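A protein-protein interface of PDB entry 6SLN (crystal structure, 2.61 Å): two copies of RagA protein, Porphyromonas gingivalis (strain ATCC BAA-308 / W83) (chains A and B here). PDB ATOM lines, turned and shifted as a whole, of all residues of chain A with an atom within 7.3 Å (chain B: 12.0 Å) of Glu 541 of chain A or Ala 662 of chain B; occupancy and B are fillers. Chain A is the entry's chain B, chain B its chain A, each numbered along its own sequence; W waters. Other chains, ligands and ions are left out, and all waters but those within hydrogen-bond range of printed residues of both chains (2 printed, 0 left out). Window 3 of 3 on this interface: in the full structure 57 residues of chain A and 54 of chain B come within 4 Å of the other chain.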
ATOM      1  N   PRO A 477      23.544  14.551  -8.378  1.00  0.00           N
ATOM      2  CA  PRO A 477      22.126  14.253  -8.644  1.00  0.00           C
ATOM      3  C   PRO A 477      21.858  12.767  -8.858  1.00  0.00           C
ATOM      4  O   PRO A 477      22.760  11.966  -9.111  1.00  0.00           O
ATOM      5  CB  PRO A 477      21.830  15.028  -9.939  1.00  0.00           C
ATOM      6  CG  PRO A 477      23.149  15.066 -10.653  1.00  0.00           C
ATOM      7  CD  PRO A 477      24.204  15.200  -9.524  1.00  0.00           C
ATOM      8  N   ASN A 478      20.571  12.419  -8.773  1.00  0.00           N
ATOM      9  CA  ASN A 478      20.078  11.100  -9.165  1.00  0.00           C
ATOM     10  C   ASN A 478      20.656   9.992  -8.296  1.00  0.00           C
ATOM     11  O   ASN A 478      20.752   8.844  -8.723  1.00  0.00           O
ATOM     12  CB  ASN A 478      20.378  10.813 -10.642  1.00  0.00           C
ATOM     13  CG  ASN A 478      19.593  11.692 -11.571  1.00  0.00           C
ATOM     14  OD1 ASN A 478      18.366  11.758 -11.495  1.00  0.00           O
ATOM     15  ND2 ASN A 478      20.294  12.382 -12.453  1.00  0.00           N
ATOM     16  N   PRO A 485      16.625  13.562  -5.633  1.00  0.00           N
ATOM     17  CA  PRO A 485      17.398  13.296  -6.855  1.00  0.00           C
ATOM     18  C   PRO A 485      18.110  14.530  -7.358  1.00  0.00           C
ATOM     19  O   PRO A 485      19.052  14.404  -8.149  1.00  0.00           O
ATOM     20  CB  PRO A 485      16.335  12.822  -7.841  1.00  0.00           C
ATOM     21  CG  PRO A 485      15.101  13.560  -7.409  1.00  0.00           C
ATOM     22  CD  PRO A 485      15.171  13.564  -5.888  1.00  0.00           C
ATOM     23  N   LEU A 486      17.696  15.713  -6.909  1.00  0.00           N
ATOM     24  CA  LEU A 486      18.267  16.959  -7.393  1.00  0.00           C
ATOM     25  C   LEU A 486      19.638  17.178  -6.779  1.00  0.00           C
ATOM     26  O   LEU A 486      19.830  16.982  -5.583  1.00  0.00           O
ATOM     27  CB  LEU A 486      17.353  18.131  -7.051  1.00  0.00           C
ATOM     28  CG  LEU A 486      15.968  17.969  -7.667  1.00  0.00           C
ATOM     29  CD1 LEU A 486      15.111  19.185  -7.374  1.00  0.00           C
ATOM     30  CD2 LEU A 486      16.078  17.688  -9.176  1.00  0.00           C
ATOM     31  N   GLY A 487      20.599  17.568  -7.609  1.00  0.00           N
ATOM     32  CA  GLY A 487      21.933  17.866  -7.144  1.00  0.00           C
ATOM     33  C   GLY A 487      22.137  19.329  -6.726  1.00  0.00           C
ATOM     34  O   GLY A 487      21.251  20.177  -6.803  1.00  0.00           O
ATOM     35  N   LYS A 538      21.216  24.644  -6.860  1.00  0.00           N
ATOM     36  CA  LYS A 538      20.715  23.299  -6.671  1.00  0.00           C
ATOM     37  C   LYS A 538      19.539  23.039  -7.599  1.00  0.00           C
ATOM     38  O   LYS A 538      19.153  23.879  -8.407  1.00  0.00           O
ATOM     39  CB  LYS A 538      20.354  23.079  -5.207  1.00  0.00           C
ATOM     40  CG  LYS A 538      19.282  23.991  -4.712  1.00  0.00           C
ATOM     41  CD  LYS A 538      19.173  23.858  -3.221  1.00  0.00           C
ATOM     42  CE  LYS A 538      18.256  24.927  -2.651  1.00  0.00           C
ATOM     43  NZ  LYS A 538      18.426  25.052  -1.184  1.00  0.00           N
ATOM     44  N   GLY A 539      18.984  21.837  -7.489  1.00  0.00           N
ATOM     45  CA  GLY A 539      17.995  21.369  -8.434  1.00  0.00           C
ATOM     46  C   GLY A 539      18.562  20.782  -9.697  1.00  0.00           C
ATOM     47  O   GLY A 539      17.811  20.599 -10.660  1.00  0.00           O
ATOM     48  N   PHE A 540      19.860  20.497  -9.742  1.00  0.00           N
ATOM     49  CA  PHE A 540      20.434  19.879 -10.933  1.00  0.00           C
ATOM     50  C   PHE A 540      19.872  18.469 -11.146  1.00  0.00           C
ATOM     51  O   PHE A 540      19.682  17.700 -10.197  1.00  0.00           O
ATOM     52  CB  PHE A 540      21.952  19.824 -10.818  1.00  0.00           C
ATOM     53  CG  PHE A 540      22.597  21.168 -10.691  1.00  0.00           C
ATOM     54  CD1 PHE A 540      22.456  22.122 -11.691  1.00  0.00           C
ATOM     55  CD2 PHE A 540      23.338  21.496  -9.562  1.00  0.00           C
ATOM     56  CE1 PHE A 540      23.054  23.372 -11.582  1.00  0.00           C
ATOM     57  CE2 PHE A 540      23.933  22.759  -9.437  1.00  0.00           C
ATOM     58  CZ  PHE A 540      23.790  23.690 -10.456  1.00  0.00           C
ATOM     59  N   GLU A 541      19.580  18.137 -12.405  1.00  0.00           N
ATOM     60  CA  GLU A 541      18.978  16.853 -12.743  1.00  0.00           C
ATOM     61  C   GLU A 541      19.896  15.993 -13.601  1.00  0.00           C
ATOM     62  O   GLU A 541      19.501  14.900 -14.029  1.00  0.00           O
ATOM     63  CB  GLU A 541      17.627  17.068 -13.430  1.00  0.00           C
ATOM     64  CG  GLU A 541      16.645  17.915 -12.632  1.00  0.00           C
ATOM     65  CD  GLU A 541      15.207  17.858 -13.156  1.00  0.00           C
ATOM     66  OE1 GLU A 541      14.323  18.537 -12.576  1.00  0.00           O
ATOM     67  OE2 GLU A 541      14.955  17.138 -14.153  1.00  0.00           O
ATOM     68  N   SER A 542      21.132  16.433 -13.822  1.00  0.00           N
ATOM     69  CA  SER A 542      22.051  15.707 -14.688  1.00  0.00           C
ATOM     70  C   SER A 542      23.468  16.074 -14.305  1.00  0.00           C
ATOM     71  O   SER A 542      23.806  17.262 -14.241  1.00  0.00           O
ATOM     72  CB  SER A 542      21.816  16.051 -16.164  1.00  0.00           C
ATOM     73  OG  SER A 542      22.996  15.808 -16.921  1.00  0.00           O
ATOM     74  N   ASP A 543      24.299  15.065 -14.067  1.00  0.00           N
ATOM     75  CA  ASP A 543      25.661  15.371 -13.676  1.00  0.00           C
ATOM     76  C   ASP A 543      26.428  16.057 -14.792  1.00  0.00           C
ATOM     77  O   ASP A 543      27.415  16.744 -14.513  1.00  0.00           O
ATOM     78  CB  ASP A 543      26.403  14.120 -13.196  1.00  0.00           C
ATOM     79  CG  ASP A 543      26.448  13.032 -14.225  1.00  0.00           C
ATOM     80  OD1 ASP A 543      25.359  12.537 -14.603  1.00  0.00           O
ATOM     81  OD2 ASP A 543      27.573  12.663 -14.644  1.00  0.00           O
ATOM     82  N   LYS A 544      25.968  15.949 -16.039  1.00  0.00           N
ATOM     83  CA  LYS A 544      26.637  16.650 -17.138  1.00  0.00           C
ATOM     84  C   LYS A 544      26.240  18.117 -17.234  1.00  0.00           C
ATOM     85  O   LYS A 544      26.911  18.877 -17.943  1.00  0.00           O
ATOM     86  CB  LYS A 544      26.357  15.933 -18.469  1.00  0.00           C
ATOM     87  CG  LYS A 544      27.093  14.598 -18.609  1.00  0.00           C
ATOM     88  CD  LYS A 544      28.504  14.784 -19.137  1.00  0.00           C
ATOM     89  CE  LYS A 544      28.474  15.403 -20.548  1.00  0.00           C
ATOM     90  NZ  LYS A 544      29.808  15.395 -21.236  1.00  0.00           N
ATOM     91  N   LEU A 545      25.194  18.543 -16.524  1.00  0.00           N
ATOM     92  CA  LEU A 545      24.661  19.907 -16.611  1.00  0.00           C
ATOM     93  C   LEU A 545      24.644  20.548 -15.217  1.00  0.00           C
ATOM     94  O   LEU A 545      23.586  20.682 -14.588  1.00  0.00           O
ATOM     95  CB  LEU A 545      23.252  19.875 -17.253  1.00  0.00           C
ATOM     96  CG  LEU A 545      23.151  19.084 -18.552  1.00  0.00           C
ATOM     97  CD1 LEU A 545      21.710  18.972 -18.988  1.00  0.00           C
ATOM     98  CD2 LEU A 545      24.003  19.790 -19.582  1.00  0.00           C
ATOM     99  N   MET A 546      25.821  20.983 -14.754  1.00  0.00           N
ATOM    100  CA  MET A 546      25.977  21.403 -13.363  1.00  0.00           C
ATOM    101  C   MET A 546      26.751  22.714 -13.230  1.00  0.00           C
ATOM    102  O   MET A 546      27.445  22.928 -12.236  1.00  0.00           O
ATOM    103  CB  MET A 546      26.657  20.306 -12.545  1.00  0.00           C
ATOM    104  CG  MET A 546      25.790  19.108 -12.320  1.00  0.00           C
ATOM    105  SD  MET A 546      26.359  18.221 -10.890  1.00  0.00           S
ATOM    106  CE  MET A 546      27.797  17.408 -11.569  1.00  0.00           C
ATOM    107  N   GLN A 550      23.057  26.974 -14.081  1.00  0.00           N
ATOM    108  CA  GLN A 550      22.021  26.068 -14.551  1.00  0.00           C
ATOM    109  C   GLN A 550      21.127  25.536 -13.448  1.00  0.00           C
ATOM    110  O   GLN A 550      20.310  24.653 -13.716  1.00  0.00           O
ATOM    111  CB  GLN A 550      22.656  24.917 -15.304  1.00  0.00           C
ATOM    112  CG  GLN A 550      23.414  25.462 -16.462  1.00  0.00           C
ATOM    113  CD  GLN A 550      24.116  24.399 -17.212  1.00  0.00           C
ATOM    114  OE1 GLN A 550      24.956  23.691 -16.654  1.00  0.00           O
ATOM    115  NE2 GLN A 550      23.780  24.258 -18.489  1.00  0.00           N
ATOM    116  N   LYS A 552      18.093  25.611 -10.481  1.00  0.00           N
ATOM    117  CA  LYS A 552      16.718  26.086 -10.497  1.00  0.00           C
ATOM    118  C   LYS A 552      16.624  27.471  -9.851  1.00  0.00           C
ATOM    119  O   LYS A 552      17.409  27.820  -8.960  1.00  0.00           O
ATOM    120  CB  LYS A 552      15.797  25.084  -9.786  1.00  0.00           C
ATOM    121  CG  LYS A 552      15.838  23.678 -10.348  1.00  0.00           C
ATOM    122  CD  LYS A 552      14.559  22.912 -10.054  1.00  0.00           C
ATOM    123  CE  LYS A 552      14.472  21.567 -10.786  1.00  0.00           C
ATOM    124  NZ  LYS A 552      15.563  21.361 -11.760  1.00  0.00           N
ATOM    125  N   LEU B 559      20.601  33.561  -9.930  1.00  0.00           N
ATOM    126  CA  LEU B 559      21.553  32.474 -10.093  1.00  0.00           C
ATOM    127  C   LEU B 559      22.959  33.042 -10.132  1.00  0.00           C
ATOM    128  O   LEU B 559      23.154  34.177 -10.537  1.00  0.00           O
ATOM    129  CB  LEU B 559      21.292  31.711 -11.375  1.00  0.00           C
ATOM    130  CG  LEU B 559      20.089  30.779 -11.325  1.00  0.00           C
ATOM    131  CD1 LEU B 559      19.688  30.376 -12.759  1.00  0.00           C
ATOM    132  CD2 LEU B 559      20.416  29.565 -10.481  1.00  0.00           C
ATOM    133  N   VAL B 653      23.261  19.905 -26.326  1.00  0.00           N
ATOM    134  CA  VAL B 653      22.061  20.391 -25.667  1.00  0.00           C
ATOM    135  C   VAL B 653      22.503  21.082 -24.389  1.00  0.00           C
ATOM    136  O   VAL B 653      23.613  20.879 -23.888  1.00  0.00           O
ATOM    137  CB  VAL B 653      21.038  19.273 -25.371  1.00  0.00           C
ATOM    138  CG1 VAL B 653      20.696  18.515 -26.662  1.00  0.00           C
ATOM    139  CG2 VAL B 653      21.567  18.331 -24.300  1.00  0.00           C
ATOM    140  N   THR B 654      21.627  21.930 -23.871  1.00  0.00           N
ATOM    141  CA  THR B 654      21.968  22.706 -22.694  1.00  0.00           C
ATOM    142  C   THR B 654      20.703  22.956 -21.893  1.00  0.00           C
ATOM    143  O   THR B 654      19.586  22.694 -22.350  1.00  0.00           O
ATOM    144  CB  THR B 654      22.674  24.026 -23.069  1.00  0.00           C
ATOM    145  OG1 THR B 654      23.495  24.464 -21.980  1.00  0.00           O
ATOM    146  CG2 THR B 654      21.666  25.129 -23.438  1.00  0.00           C
ATOM    147  N   VAL B 655      20.901  23.450 -20.674  1.00  0.00           N
ATOM    148  CA  VAL B 655      19.784  23.689 -19.781  1.00  0.00           C
ATOM    149  C   VAL B 655      19.004  24.895 -20.278  1.00  0.00           C
ATOM    150  O   VAL B 655      19.570  25.892 -20.745  1.00  0.00           O
ATOM    151  CB  VAL B 655      20.286  23.851 -18.331  1.00  0.00           C
ATOM    152  CG1 VAL B 655      19.182  24.365 -17.395  1.00  0.00           C
ATOM    153  CG2 VAL B 655      20.772  22.489 -17.820  1.00  0.00           C
ATOM    154  N   ASN B 656      17.691  24.774 -20.240  1.00  0.00           N
ATOM    155  CA  ASN B 656      16.780  25.817 -20.663  1.00  0.00           C
ATOM    156  C   ASN B 656      15.493  25.603 -19.890  1.00  0.00           C
ATOM    157  O   ASN B 656      14.532  25.009 -20.397  1.00  0.00           O
ATOM    158  CB  ASN B 656      16.521  25.774 -22.173  1.00  0.00           C
ATOM    159  CG  ASN B 656      16.028  27.109 -22.704  1.00  0.00           C
ATOM    160  OD1 ASN B 656      16.269  28.143 -22.086  1.00  0.00           O
ATOM    161  ND2 ASN B 656      15.349  27.096 -23.845  1.00  0.00           N
ATOM    162  N   ASN B 657      15.471  26.068 -18.660  1.00  0.00           N
ATOM    163  CA  ASN B 657      14.405  25.675 -17.765  1.00  0.00           C
ATOM    164  C   ASN B 657      13.136  26.476 -18.034  1.00  0.00           C
ATOM    165  O   ASN B 657      13.168  27.704 -18.130  1.00  0.00           O
ATOM    166  CB  ASN B 657      14.905  25.806 -16.334  1.00  0.00           C
ATOM    167  CG  ASN B 657      16.083  24.891 -16.092  1.00  0.00           C
ATOM    168  OD1 ASN B 657      16.128  23.784 -16.640  1.00  0.00           O
ATOM    169  ND2 ASN B 657      17.049  25.345 -15.342  1.00  0.00           N
ATOM    170  N   TYR B 658      12.030  25.754 -18.217  1.00  0.00           N
ATOM    171  CA  TYR B 658      10.712  26.362 -18.355  1.00  0.00           C
ATOM    172  C   TYR B 658      10.145  26.770 -16.993  1.00  0.00           C
ATOM    173  O   TYR B 658       9.948  27.958 -16.721  1.00  0.00           O
ATOM    174  CB  TYR B 658       9.771  25.393 -19.079  1.00  0.00           C
ATOM    175  CG  TYR B 658       8.462  26.029 -19.462  1.00  0.00           C
ATOM    176  CD1 TYR B 658       8.426  27.308 -19.982  1.00  0.00           C
ATOM    177  CD2 TYR B 658       7.266  25.365 -19.279  1.00  0.00           C
ATOM    178  CE1 TYR B 658       7.239  27.898 -20.316  1.00  0.00           C
ATOM    179  CE2 TYR B 658       6.070  25.948 -19.614  1.00  0.00           C
ATOM    180  CZ  TYR B 658       6.062  27.213 -20.135  1.00  0.00           C
ATOM    181  OH  TYR B 658       4.871  27.811 -20.490  1.00  0.00           O
ATOM    182  N   THR B 659       9.860  25.796 -16.122  1.00  0.00           N
ATOM    183  CA  THR B 659       9.365  26.091 -14.785  1.00  0.00           C
ATOM    184  C   THR B 659      10.516  26.063 -13.792  1.00  0.00           C
ATOM    185  O   THR B 659      11.684  25.900 -14.158  1.00  0.00           O
ATOM    186  CB  THR B 659       8.284  25.107 -14.338  1.00  0.00           C
ATOM    187  OG1 THR B 659       8.899  23.894 -13.902  1.00  0.00           O
ATOM    188  CG2 THR B 659       7.327  24.805 -15.429  1.00  0.00           C
ATOM    189  N   GLU B 660      10.186  26.200 -12.512  1.00  0.00           N
ATOM    190  CA  GLU B 660      11.178  26.089 -11.452  1.00  0.00           C
ATOM    191  C   GLU B 660      11.181  24.721 -10.783  1.00  0.00           C
ATOM    192  O   GLU B 660      11.983  24.486  -9.875  1.00  0.00           O
ATOM    193  CB  GLU B 660      10.941  27.180 -10.415  1.00  0.00           C
ATOM    194  CG  GLU B 660      11.047  28.569 -11.013  1.00  0.00           C
ATOM    195  CD  GLU B 660      10.572  29.665 -10.073  1.00  0.00           C
ATOM    196  OE1 GLU B 660       9.525  29.496  -9.388  1.00  0.00           O
ATOM    197  OE2 GLU B 660      11.250  30.712 -10.054  1.00  0.00           O
ATOM    198  N   ASP B 661      10.339  23.800 -11.235  1.00  0.00           N
ATOM    199  CA  ASP B 661      10.183  22.510 -10.590  1.00  0.00           C
ATOM    200  C   ASP B 661      10.723  21.346 -11.408  1.00  0.00           C
ATOM    201  O   ASP B 661      10.579  20.194 -10.988  1.00  0.00           O
ATOM    202  CB  ASP B 661       8.709  22.311 -10.262  1.00  0.00           C
ATOM    203  CG  ASP B 661       8.192  23.404  -9.348  1.00  0.00           C
ATOM    204  OD1 ASP B 661       9.000  23.907  -8.543  1.00  0.00           O
ATOM    205  OD2 ASP B 661       7.003  23.774  -9.429  1.00  0.00           O
ATOM    206  N   ALA B 662      11.377  21.613 -12.533  1.00  0.00           N
ATOM    207  CA  ALA B 662      11.789  20.556 -13.446  1.00  0.00           C
ATOM    208  C   ALA B 662      12.817  21.140 -14.403  1.00  0.00           C
ATOM    209  O   ALA B 662      12.860  22.353 -14.617  1.00  0.00           O
ATOM    210  CB  ALA B 662      10.584  19.975 -14.203  1.00  0.00           C
ATOM    211  N   MET B 663      13.667  20.278 -14.957  1.00  0.00           N
ATOM    212  CA  MET B 663      14.688  20.749 -15.887  1.00  0.00           C
ATOM    213  C   MET B 663      14.162  20.741 -17.325  1.00  0.00           C
ATOM    214  O   MET B 663      13.278  19.952 -17.678  1.00  0.00           O
ATOM    215  CB  MET B 663      15.960  19.904 -15.775  1.00  0.00           C
ATOM    216  CG  MET B 663      17.108  20.384 -16.650  1.00  0.00           C
ATOM    217  SD  MET B 663      18.562  19.340 -16.466  1.00  0.00           S
ATOM    218  CE  MET B 663      18.217  18.000 -17.599  1.00  0.00           C
ATOM    219  N   GLY B 664      14.686  21.673 -18.121  1.00  0.00           N
ATOM    220  CA  GLY B 664      14.330  21.763 -19.534  1.00  0.00           C
ATOM    221  C   GLY B 664      15.583  21.782 -20.384  1.00  0.00           C
ATOM    222  O   GLY B 664      16.589  22.378 -20.013  1.00  0.00           O
ATOM    223  N   LEU B 665      15.522  21.074 -21.511  1.00  0.00           N
ATOM    224  CA  LEU B 665      16.646  20.962 -22.433  1.00  0.00           C
ATOM    225  C   LEU B 665      16.321  21.615 -23.772  1.00  0.00           C
ATOM    226  O   LEU B 665      15.194  21.503 -24.275  1.00  0.00           O
ATOM    227  CB  LEU B 665      17.017  19.494 -22.652  1.00  0.00           C
ATOM    228  CG  LEU B 665      17.574  18.833 -21.403  1.00  0.00           C
ATOM    229  CD1 LEU B 665      17.748  17.336 -21.656  1.00  0.00           C
ATOM    230  CD2 LEU B 665      18.871  19.505 -21.082  1.00  0.00           C
ATOM    231  N   SER B 666      17.313  22.295 -24.349  1.00  0.00           N
ATOM    232  CA  SER B 666      17.197  22.845 -25.694  1.00  0.00           C
ATOM    233  C   SER B 666      18.467  22.548 -26.465  1.00  0.00           C
ATOM    234  O   SER B 666      19.560  22.471 -25.896  1.00  0.00           O
ATOM    235  CB  SER B 666      16.952  24.355 -25.700  1.00  0.00           C
ATOM    236  OG  SER B 666      15.658  24.639 -25.188  1.00  0.00           O
HETATM  237  O   HOH W   1      12.568  16.992 -14.786  1.00  0.00           O
HETATM  238  O   HOH W   2      22.245  26.584 -19.851  1.00  0.00           O
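The side-chain carboxylate (OE1) of Glu 541 of chain A lies within hydrogen-bond range of the backbone NH (N) of Met 663 of chain B (3.0 Å).
O of Ser 666 of chain B sits at hydrogen-bond distance from N of Thr 654 of chain B (2.9 Å).
The side-chain amide nitrogen of Asn 478 of chain A sits at hydrogen-bond distance from the backbone carbonyl oxygen of Glu 541 of chain A, at 3.1 Å.
The backbone NH (N) of Gly 664 of chain B lies within hydrogen-bond range of the side-chain amide oxygen (OD1) of Asn 657 of chain B (3.0 Å).
The backbone carbonyl oxygen (O) of Gly 539 of chain A sits at hydrogen-bond distance from the side-chain amino group (NZ) of Lys 552 of chain A.
OE1 of Glu 541 of chain A is in salt-bridge range of NZ of Lys 552 of chain A (3.2 Å).
The side-chain hydroxyl (OG1) of Thr 659 of chain B sits at hydrogen-bond distance from the backbone NH (N) of Asp 661 of chain B (3.0 Å).
Among the printed residues, pairs that only touch across the chains: Glu 541 of chain A with Ala 662 of chain B (3.4 Å), Leu 545 of chain A with Val 655 of chain B (3.6 Å), Leu 545 of chain A with Met 663 of chain B (3.9 Å), Leu 545 of chain A with Leu 665 of chain B (3.6 Å), Gln 550 of chain A with Thr 654 of chain B (3.5 Å), Gln 550 of chain A with Val 655 of chain B (3.5 Å), Gln 550 of chain A with Asn 657 of chain B (3.7 Å), Lys 552 of chain A with Leu 559 of chain B (3.8 Å), Lys 552 of chain A with Glu 660 of chain B (3.0 Å), Lys 552 of chain A with Asp 661 of chain B (3.8 Å), Lys 552 of chain A with Ala 662 of chain B (3.6 Å) and Lys 552 of chain A with Met 663 of chain B (3.9 Å).
Of chain B, only Ala 662 (3.4 Å) and Met 663 (3.0 Å) come within 4 Å of Glu 541 of chain A.
Ala 662 of chain B touches two residues of chain A.
No residue of chain B comes within 4 Å of Pro 477 of chain A.
Leu 486 of chain A touches none of the printed residues of chain B.
No residue of chain B comes within 4 Å of Gly 539 of chain A.
No residue of chain B comes within 4 Å of Phe 540 of chain A.
Printed residues of chain A within 4 Å of Leu 559 of chain B: Lys 552 (3.8 Å).
Printed residues of chain A within 4 Å of Glu 660 of chain B: Lys 552.
The nearest residue of chain B that does not touch Glu 541 of chain A is Asp 661 of chain B (4.4 Å).
The nearest printed residue of chain A that does not touch Asp 661 of chain B is Glu 541 of chain A (4.4 Å).
Printed residues of chain B that touch a printed residue of chain A: Leu 559, Thr 654, Val 655, Asn 657, Glu 660, Asp 661, Ala 662, Met 663 and Leu 665.
Hydrophobic or aromatic side chains of chain B within 4 Å of the printed part of chain A: Leu 559, Val 655, Met 663 and Leu 665.
Printed residues of chain A that touch a printed residue of chain B: Glu 541, Leu 545, Gln 550 and Lys 552.
Hydrophobic or aromatic side chains of chain A that line the printed part of chain B: Leu 545.
No position is printed for both chains.
Water W1 lies within hydrogen-bond range of OE2 of Glu 541 of chain A and N of Met 663 of chain B.
Water W2 lies within hydrogen-bond range of O of Val 655 of chain B (2.9 Å), NE2 of Gln 550 of chain A (3.1 Å) and OG1 of Thr 654 of chain B (3.3 Å).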
